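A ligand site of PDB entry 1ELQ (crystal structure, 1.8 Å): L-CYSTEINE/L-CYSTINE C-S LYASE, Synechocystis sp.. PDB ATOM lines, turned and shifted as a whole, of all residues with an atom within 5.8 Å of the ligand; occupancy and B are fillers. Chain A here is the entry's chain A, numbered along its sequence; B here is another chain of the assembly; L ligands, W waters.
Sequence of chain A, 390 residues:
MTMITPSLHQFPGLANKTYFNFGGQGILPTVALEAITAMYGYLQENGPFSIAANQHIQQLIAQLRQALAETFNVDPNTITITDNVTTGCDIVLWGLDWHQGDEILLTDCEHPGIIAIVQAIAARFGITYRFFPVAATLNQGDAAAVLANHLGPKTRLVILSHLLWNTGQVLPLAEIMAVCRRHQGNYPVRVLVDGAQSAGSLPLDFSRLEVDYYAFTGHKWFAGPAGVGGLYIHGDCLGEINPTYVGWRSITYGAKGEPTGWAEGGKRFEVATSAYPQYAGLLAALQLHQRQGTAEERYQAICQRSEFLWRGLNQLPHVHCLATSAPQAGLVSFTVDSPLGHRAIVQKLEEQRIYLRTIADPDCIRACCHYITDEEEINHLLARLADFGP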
ATOM      1  N   GLY A  23      -0.881  28.369  23.707  1.00  0.00           N
ATOM      2  CA  GLY A  23      -2.117  27.776  24.187  1.00  0.00           C
ATOM      3  C   GLY A  23      -2.426  28.227  25.621  1.00  0.00           C
ATOM      4  O   GLY A  23      -3.499  27.927  26.134  1.00  0.00           O
ATOM      5  N   GLY A  24      -1.432  28.863  26.255  1.00  0.00           N
ATOM      6  CA  GLY A  24      -1.562  29.422  27.614  1.00  0.00           C
ATOM      7  C   GLY A  24      -1.952  30.878  27.396  1.00  0.00           C
ATOM      8  O   GLY A  24      -3.008  31.354  27.875  1.00  0.00           O
ATOM      9  N   ASP A  83     -14.942  38.231  28.618  1.00  0.00           N
ATOM     10  CA  ASP A  83     -13.562  38.474  29.004  1.00  0.00           C
ATOM     11  C   ASP A  83     -12.680  37.260  28.813  1.00  0.00           C
ATOM     12  O   ASP A  83     -11.473  37.396  28.864  1.00  0.00           O
ATOM     13  CB  ASP A  83     -13.434  38.837  30.487  1.00  0.00           C
ATOM     14  CG  ASP A  83     -14.088  40.131  30.831  1.00  0.00           C
ATOM     15  OD1 ASP A  83     -14.331  40.938  29.907  1.00  0.00           O
ATOM     16  OD2 ASP A  83     -14.345  40.355  32.044  1.00  0.00           O
ATOM     17  N   ASN A  84     -13.267  36.071  28.602  1.00  0.00           N
ATOM     18  CA  ASN A  84     -12.456  34.843  28.524  1.00  0.00           C
ATOM     19  C   ASN A  84     -13.332  33.647  28.097  1.00  0.00           C
ATOM     20  O   ASN A  84     -14.531  33.766  27.975  1.00  0.00           O
ATOM     21  CB  ASN A  84     -11.862  34.557  29.908  1.00  0.00           C
ATOM     22  CG  ASN A  84     -12.894  34.662  31.012  1.00  0.00           C
ATOM     23  OD1 ASN A  84     -13.959  34.077  30.919  1.00  0.00           O
ATOM     24  ND2 ASN A  84     -12.584  35.420  32.066  1.00  0.00           N
ATOM     25  N   VAL A  85     -12.729  32.479  27.896  1.00  0.00           N
ATOM     26  CA  VAL A  85     -13.510  31.321  27.498  1.00  0.00           C
ATOM     27  C   VAL A  85     -14.574  30.936  28.521  1.00  0.00           C
ATOM     28  O   VAL A  85     -15.747  30.718  28.201  1.00  0.00           O
ATOM     29  CB  VAL A  85     -12.579  30.089  27.293  1.00  0.00           C
ATOM     30  CG1 VAL A  85     -13.390  28.862  26.922  1.00  0.00           C
ATOM     31  CG2 VAL A  85     -11.540  30.421  26.227  1.00  0.00           C
ATOM     32  N   THR A  86     -14.153  30.850  29.779  1.00  0.00           N
ATOM     33  CA  THR A  86     -15.004  30.409  30.859  1.00  0.00           C
ATOM     34  C   THR A  86     -16.338  31.129  30.966  1.00  0.00           C
ATOM     35  O   THR A  86     -17.364  30.480  31.104  1.00  0.00           O
ATOM     36  CB  THR A  86     -14.218  30.450  32.197  1.00  0.00           C
ATOM     37  OG1 THR A  86     -13.039  29.660  32.041  1.00  0.00           O
ATOM     38  CG2 THR A  86     -15.075  29.862  33.369  1.00  0.00           C
ATOM     39  N   THR A  87     -16.321  32.459  30.900  1.00  0.00           N
ATOM     40  CA  THR A  87     -17.547  33.255  31.000  1.00  0.00           C
ATOM     41  C   THR A  87     -18.551  32.798  29.915  1.00  0.00           C
ATOM     42  O   THR A  87     -19.737  32.737  30.168  1.00  0.00           O
ATOM     43  CB  THR A  87     -17.204  34.764  30.885  1.00  0.00           C
ATOM     44  OG1 THR A  87     -16.424  35.153  32.039  1.00  0.00           O
ATOM     45  CG2 THR A  87     -18.487  35.618  30.809  1.00  0.00           C
ATOM     46  N   CYS A 109     -11.422  15.145  29.244  1.00  0.00           N
ATOM     47  CA  CYS A 109     -10.337  16.071  28.918  1.00  0.00           C
ATOM     48  C   CYS A 109     -10.741  17.552  29.058  1.00  0.00           C
ATOM     49  O   CYS A 109     -10.124  18.451  28.470  1.00  0.00           O
ATOM     50  CB  CYS A 109      -9.813  15.787  27.505  1.00  0.00           C
ATOM     51  SG  CYS A 109      -8.867  14.263  27.398  1.00  0.00           S
ATOM     52  N   GLU A 110     -11.750  17.823  29.880  1.00  0.00           N
ATOM     53  CA  GLU A 110     -12.192  19.209  30.004  1.00  0.00           C
ATOM     54  C   GLU A 110     -11.434  19.972  31.070  1.00  0.00           C
ATOM     55  O   GLU A 110     -10.823  19.405  31.974  1.00  0.00           O
ATOM     56  CB  GLU A 110     -13.706  19.276  30.246  1.00  0.00           C
ATOM     57  CG  GLU A 110     -14.551  18.606  29.119  1.00  0.00           C
ATOM     58  CD  GLU A 110     -14.186  19.077  27.721  1.00  0.00           C
ATOM     59  OE1 GLU A 110     -14.135  20.309  27.480  1.00  0.00           O
ATOM     60  OE2 GLU A 110     -13.973  18.224  26.818  1.00  0.00           O
ATOM     61  N   HIS A 111     -11.507  21.296  30.942  1.00  0.00           N
ATOM     62  CA  HIS A 111     -10.802  22.218  31.835  1.00  0.00           C
ATOM     63  C   HIS A 111     -11.411  22.137  33.213  1.00  0.00           C
ATOM     64  O   HIS A 111     -12.639  22.092  33.362  1.00  0.00           O
ATOM     65  CB  HIS A 111     -10.952  23.631  31.281  1.00  0.00           C
ATOM     66  CG  HIS A 111      -9.920  24.580  31.788  1.00  0.00           C
ATOM     67  ND1 HIS A 111      -8.687  24.731  31.185  1.00  0.00           N
ATOM     68  CD2 HIS A 111      -9.928  25.425  32.847  1.00  0.00           C
ATOM     69  CE1 HIS A 111      -7.980  25.629  31.850  1.00  0.00           C
ATOM     70  NE2 HIS A 111      -8.711  26.068  32.865  1.00  0.00           N
ATOM     71  N   ILE A 114     -14.285  24.530  33.956  1.00  0.00           N
ATOM     72  CA  ILE A 114     -15.582  24.213  33.320  1.00  0.00           C
ATOM     73  C   ILE A 114     -16.300  23.111  34.097  1.00  0.00           C
ATOM     74  O   ILE A 114     -17.530  23.087  34.163  1.00  0.00           O
ATOM     75  CB  ILE A 114     -15.390  23.843  31.820  1.00  0.00           C
ATOM     76  CG1 ILE A 114     -15.411  25.112  30.948  1.00  0.00           C
ATOM     77  CG2 ILE A 114     -16.550  23.035  31.319  1.00  0.00           C
ATOM     78  CD1 ILE A 114     -14.349  26.093  31.204  1.00  0.00           C
ATOM     79  N   SER A 161     -14.188  19.967  24.348  1.00  0.00           N
ATOM     80  CA  SER A 161     -13.232  20.931  23.812  1.00  0.00           C
ATOM     81  C   SER A 161     -12.978  20.503  22.379  1.00  0.00           C
ATOM     82  O   SER A 161     -12.691  19.338  22.110  1.00  0.00           O
ATOM     83  CB  SER A 161     -11.945  20.876  24.610  1.00  0.00           C
ATOM     84  OG  SER A 161     -12.166  21.425  25.897  1.00  0.00           O
ATOM     85  N   LEU A 163     -10.480  21.234  20.535  1.00  0.00           N
ATOM     86  CA  LEU A 163      -9.097  20.813  20.479  1.00  0.00           C
ATOM     87  C   LEU A 163      -8.769  20.616  21.965  1.00  0.00           C
ATOM     88  O   LEU A 163      -8.904  21.553  22.738  1.00  0.00           O
ATOM     89  CB  LEU A 163      -8.256  21.933  19.857  1.00  0.00           C
ATOM     90  CG  LEU A 163      -6.966  21.637  19.059  1.00  0.00           C
ATOM     91  CD1 LEU A 163      -6.153  22.926  18.940  1.00  0.00           C
ATOM     92  CD2 LEU A 163      -6.147  20.529  19.656  1.00  0.00           C
ATOM     93  N   LEU A 164      -8.348  19.409  22.351  1.00  0.00           N
ATOM     94  CA  LEU A 164      -8.078  19.107  23.771  1.00  0.00           C
ATOM     95  C   LEU A 164      -6.834  19.815  24.259  1.00  0.00           C
ATOM     96  O   LEU A 164      -5.785  19.697  23.656  1.00  0.00           O
ATOM     97  CB  LEU A 164      -7.958  17.581  23.982  1.00  0.00           C
ATOM     98  CG  LEU A 164      -9.161  16.723  23.513  1.00  0.00           C
ATOM     99  CD1 LEU A 164      -8.907  15.255  23.852  1.00  0.00           C
ATOM    100  CD2 LEU A 164     -10.465  17.203  24.118  1.00  0.00           C
ATOM    101  N   TRP A 165      -6.951  20.589  25.336  1.00  0.00           N
ATOM    102  CA  TRP A 165      -5.812  21.332  25.863  1.00  0.00           C
ATOM    103  C   TRP A 165      -4.707  20.431  26.432  1.00  0.00           C
ATOM    104  O   TRP A 165      -3.576  20.879  26.625  1.00  0.00           O
ATOM    105  CB  TRP A 165      -6.312  22.275  26.976  1.00  0.00           C
ATOM    106  CG  TRP A 165      -6.523  21.611  28.324  1.00  0.00           C
ATOM    107  CD1 TRP A 165      -7.168  20.428  28.585  1.00  0.00           C
ATOM    108  CD2 TRP A 165      -6.132  22.139  29.591  1.00  0.00           C
ATOM    109  NE1 TRP A 165      -7.202  20.190  29.955  1.00  0.00           N
ATOM    110  CE2 TRP A 165      -6.572  21.229  30.584  1.00  0.00           C
ATOM    111  CE3 TRP A 165      -5.457  23.301  29.987  1.00  0.00           C
ATOM    112  CZ2 TRP A 165      -6.346  21.450  31.954  1.00  0.00           C
ATOM    113  CZ3 TRP A 165      -5.252  23.527  31.344  1.00  0.00           C
ATOM    114  CH2 TRP A 165      -5.692  22.592  32.314  1.00  0.00           C
ATOM    115  N   ASP A 194     -16.002  24.103  24.045  1.00  0.00           N
ATOM    116  CA  ASP A 194     -14.987  24.943  24.661  1.00  0.00           C
ATOM    117  C   ASP A 194     -13.931  25.060  23.542  1.00  0.00           C
ATOM    118  O   ASP A 194     -13.191  24.100  23.290  1.00  0.00           O
ATOM    119  CB  ASP A 194     -14.391  24.244  25.878  1.00  0.00           C
ATOM    120  CG  ASP A 194     -13.212  24.993  26.467  1.00  0.00           C
ATOM    121  OD1 ASP A 194     -12.843  24.705  27.645  1.00  0.00           O
ATOM    122  OD2 ASP A 194     -12.615  25.851  25.788  1.00  0.00           O
ATOM    123  N   ALA A 196     -11.188  27.009  23.428  1.00  0.00           N
ATOM    124  CA  ALA A 196      -9.994  27.711  23.907  1.00  0.00           C
ATOM    125  C   ALA A 196      -8.753  27.475  23.052  1.00  0.00           C
ATOM    126  O   ALA A 196      -7.939  28.392  22.868  1.00  0.00           O
ATOM    127  CB  ALA A 196      -9.705  27.306  25.305  1.00  0.00           C
ATOM    128  N   GLN A 197      -8.596  26.256  22.555  1.00  0.00           N
ATOM    129  CA  GLN A 197      -7.437  25.919  21.729  1.00  0.00           C
ATOM    130  C   GLN A 197      -7.760  26.021  20.239  1.00  0.00           C
ATOM    131  O   GLN A 197      -6.924  26.436  19.429  1.00  0.00           O
ATOM    132  CB  GLN A 197      -6.964  24.499  22.062  1.00  0.00           C
ATOM    133  CG  GLN A 197      -6.579  24.305  23.536  1.00  0.00           C
ATOM    134  CD  GLN A 197      -5.471  25.259  23.966  1.00  0.00           C
ATOM    135  OE1 GLN A 197      -4.559  25.537  23.201  1.00  0.00           O
ATOM    136  NE2 GLN A 197      -5.558  25.769  25.215  1.00  0.00           N
ATOM    137  N   THR A 217     -11.790  32.546  23.515  1.00  0.00           N
ATOM    138  CA  THR A 217     -11.124  33.699  24.076  1.00  0.00           C
ATOM    139  C   THR A 217     -10.236  34.309  23.025  1.00  0.00           C
ATOM    140  O   THR A 217      -9.889  33.665  22.016  1.00  0.00           O
ATOM    141  CB  THR A 217     -10.248  33.331  25.344  1.00  0.00           C
ATOM    142  OG1 THR A 217      -9.754  34.546  25.912  1.00  0.00           O
ATOM    143  CG2 THR A 217      -9.025  32.443  24.959  1.00  0.00           C
ATOM    144  N   HIS A 219      -7.283  35.731  23.948  1.00  0.00           N
ATOM    145  CA  HIS A 219      -5.909  35.824  24.417  1.00  0.00           C
ATOM    146  C   HIS A 219      -4.976  34.660  24.174  1.00  0.00           C
ATOM    147  O   HIS A 219      -3.839  34.708  24.594  1.00  0.00           O
ATOM    148  CB  HIS A 219      -5.893  36.210  25.922  1.00  0.00           C
ATOM    149  CG  HIS A 219      -6.126  35.067  26.860  1.00  0.00           C
ATOM    150  ND1 HIS A 219      -7.373  34.525  27.082  1.00  0.00           N
ATOM    151  CD2 HIS A 219      -5.266  34.379  27.654  1.00  0.00           C
ATOM    152  CE1 HIS A 219      -7.273  33.547  27.956  1.00  0.00           C
ATOM    153  NE2 HIS A 219      -6.007  33.431  28.314  1.00  0.00           N
ATOM    154  N   LYS A 220      -5.443  33.596  23.513  1.00  0.00           N
ATOM    155  CA  LYS A 220      -4.553  32.495  23.243  1.00  0.00           C
ATOM    156  C   LYS A 220      -4.124  32.511  21.783  1.00  0.00           C
ATOM    157  O   LYS A 220      -3.303  33.342  21.408  1.00  0.00           O
ATOM    158  CB  LYS A 220      -5.198  31.161  23.641  1.00  0.00           C
ATOM    159  CG  LYS A 220      -5.302  31.089  25.192  1.00  0.00           C
ATOM    160  CD  LYS A 220      -6.095  29.865  25.629  1.00  0.00           C
ATOM    161  CE  LYS A 220      -6.096  29.814  27.151  1.00  0.00           C
ATOM    162  NZ  LYS A 220      -7.144  28.863  27.540  1.00  0.00           N
ATOM    163  N   ARG A 366       3.476  19.893  27.359  1.00  0.00           N
ATOM    164  CA  ARG A 366       2.827  20.349  26.132  1.00  0.00           C
ATOM    165  C   ARG A 366       3.553  21.529  25.528  1.00  0.00           C
ATOM    166  O   ARG A 366       3.935  22.483  26.234  1.00  0.00           O
ATOM    167  CB  ARG A 366       1.377  20.773  26.403  1.00  0.00           C
ATOM    168  CG  ARG A 366       0.554  21.183  25.161  1.00  0.00           C
ATOM    169  CD  ARG A 366      -0.731  21.908  25.580  1.00  0.00           C
ATOM    170  NE  ARG A 366      -0.419  23.248  26.063  1.00  0.00           N
ATOM    171  CZ  ARG A 366      -1.285  24.056  26.678  1.00  0.00           C
ATOM    172  NH1 ARG A 366      -2.531  23.672  26.911  1.00  0.00           N
ATOM    173  NH2 ARG A 366      -0.902  25.262  27.021  1.00  0.00           N
ATOM    174  N   TRP B 248     -11.630  28.702  36.630  1.00  0.00           N
ATOM    175  CA  TRP B 248     -10.431  28.192  37.246  1.00  0.00           C
ATOM    176  C   TRP B 248      -9.901  28.997  38.423  1.00  0.00           C
ATOM    177  O   TRP B 248      -9.184  28.459  39.241  1.00  0.00           O
ATOM    178  CB  TRP B 248      -9.325  27.921  36.188  1.00  0.00           C
ATOM    179  CG  TRP B 248      -8.897  29.088  35.370  1.00  0.00           C
ATOM    180  CD1 TRP B 248      -9.395  29.482  34.149  1.00  0.00           C
ATOM    181  CD2 TRP B 248      -7.892  30.043  35.713  1.00  0.00           C
ATOM    182  NE1 TRP B 248      -8.747  30.614  33.725  1.00  0.00           N
ATOM    183  CE2 TRP B 248      -7.823  30.986  34.671  1.00  0.00           C
ATOM    184  CE3 TRP B 248      -7.034  30.187  36.816  1.00  0.00           C
ATOM    185  CZ2 TRP B 248      -6.932  32.069  34.691  1.00  0.00           C
ATOM    186  CZ3 TRP B 248      -6.150  31.263  36.838  1.00  0.00           C
ATOM    187  CH2 TRP B 248      -6.104  32.195  35.780  1.00  0.00           C
ATOM    188  N   ALA B 272     -11.987  33.784  35.705  1.00  0.00           N
ATOM    189  CA  ALA B 272     -10.896  33.279  34.882  1.00  0.00           C
ATOM    190  C   ALA B 272     -10.036  34.400  34.325  1.00  0.00           C
ATOM    191  O   ALA B 272      -9.858  35.416  34.971  1.00  0.00           O
ATOM    192  CB  ALA B 272     -11.449  32.401  33.745  1.00  0.00           C
ATOM    193  N   THR B 273      -9.503  34.239  33.121  1.00  0.00           N
ATOM    194  CA  THR B 273      -8.597  35.287  32.625  1.00  0.00           C
ATOM    195  C   THR B 273      -9.199  36.699  32.576  1.00  0.00           C
ATOM    196  O   THR B 273     -10.268  36.907  32.030  1.00  0.00           O
ATOM    197  CB  THR B 273      -8.014  34.909  31.261  1.00  0.00           C
ATOM    198  OG1 THR B 273      -7.305  33.673  31.380  1.00  0.00           O
ATOM    199  CG2 THR B 273      -7.030  35.975  30.814  1.00  0.00           C
HETATM  200  N1  LIG L   1     -10.695  25.655  28.473  1.00  0.00           N
HETATM  201  C1  LIG L   1      -9.553  25.155  27.789  1.00  0.00           C
HETATM  202  C2  LIG L   1      -9.791  23.889  26.963  1.00  0.00           C
HETATM  203  C3  LIG L   1      -8.361  25.991  27.857  1.00  0.00           C
HETATM  204  O1  LIG L   1      -7.275  25.507  27.198  1.00  0.00           O
HETATM  205  C4  LIG L   1      -8.395  27.196  28.565  1.00  0.00           C
HETATM  206  C5  LIG L   1      -7.180  27.987  28.512  1.00  0.00           C
HETATM  207  C6  LIG L   1      -9.654  27.602  29.265  1.00  0.00           C
HETATM  208  C7  LIG L   1     -10.803  26.829  29.193  1.00  0.00           C
HETATM  209  C8  LIG L   1      -9.600  28.853  30.171  1.00  0.00           C
HETATM  210  O2  LIG L   1      -9.664  30.042  29.428  1.00  0.00           O
HETATM  211  P1  LIG L   1     -10.019  31.441  30.141  1.00  0.00           P
HETATM  212  O3  LIG L   1      -9.002  31.735  31.206  1.00  0.00           O
HETATM  213  O4  LIG L   1     -11.380  31.154  30.615  1.00  0.00           O
HETATM  214  O5  LIG L   1      -9.942  32.319  28.921  1.00  0.00           O
HETATM  215  O   HOH W   1      -9.496  20.464  26.502  1.00  0.00           O
HETATM  216  O   HOH W   2      -6.753  30.417  30.787  1.00  0.00           O
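ND1 of His 111 lies close to N1 of the ligand (3.5 Å).
The backbone NH (N) of Val 85 sits close to an oxygen (O5) of the ligand.
NE1 of Trp 248 of chain B lies close to O3 of the ligand (2.8 Å).
The side-chain hydroxyl (OG1) of Thr 273 of chain B sits close to an oxygen (O3) of the ligand, at 2.6 Å.
N1 of the ligand lies close to OD1 of Asp 194, at 2.5 Å.
The side-chain amide nitrogen (NE2) of Gln 197 sits close to an oxygen (O1) of the ligand (2.6 Å).
A carbon (C5) of the ligand is covalently linked to the side-chain amino group of Lys 220.
O4 of the ligand sits close to OG1 of Thr 86.
The backbone NH (N) of Thr 86 sits close to an oxygen (O4) of the ligand, 2.9 Å away.
An oxygen (O3) of the ligand lies close to the backbone NH (N) of Thr 273 of chain B (3.2 Å).
OG of Ser 161 sits at hydrogen-bond distance from OE1 of Glu 110 (2.8 Å).
The backbone NH (N) of Thr 86 sits close to the side-chain amide oxygen (OD1) of Asn 84 (3.4 Å).
The side-chain amide oxygen (OD1) of Asn 84 sits at hydrogen-bond distance from the backbone NH (N) of Thr 87.
A ring nitrogen (NE2) of His 219 sits at hydrogen-bond distance from the side-chain hydroxyl (OG1) of Thr 273 of chain B, 3.3 Å away.
The side-chain carboxylate (OD2) of Asp 194 is in hydrogen-bond range of the backbone NH (N) of Ala 196 (3.0 Å).
O of Trp 165 sits at hydrogen-bond distance from NH1 of Arg 366 (3.0 Å).
The side-chain amide nitrogen (ND2) of Asn 84 sits at hydrogen-bond distance from the backbone carbonyl oxygen (O) of Thr 273 of chain B.
The side-chain amide nitrogen of Gln 197 lies within hydrogen-bond range of the backbone carbonyl oxygen of Gly 23 (3.1 Å).
Residues that only touch the ligand: Asn 84, Ser 161, Trp 165, Ala 196, Thr 217, His 219 and Ala 272 of chain B.
Hydrophobic or aromatic side chains within 4 Å of the ligand: Val 85, His 111, Trp 165, Ala 196, His 219, Trp 248 of chain B and Ala 272 of chain B.
The nearest printed residue that does not touch the ligand is Ile 114 (4.1 Å).
Water W1 lies within hydrogen-bond range of the backbone NH (N) of Trp 165, the backbone carbonyl oxygen (O) of Cys 109 and the side-chain hydroxyl (OG) of Ser 161.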
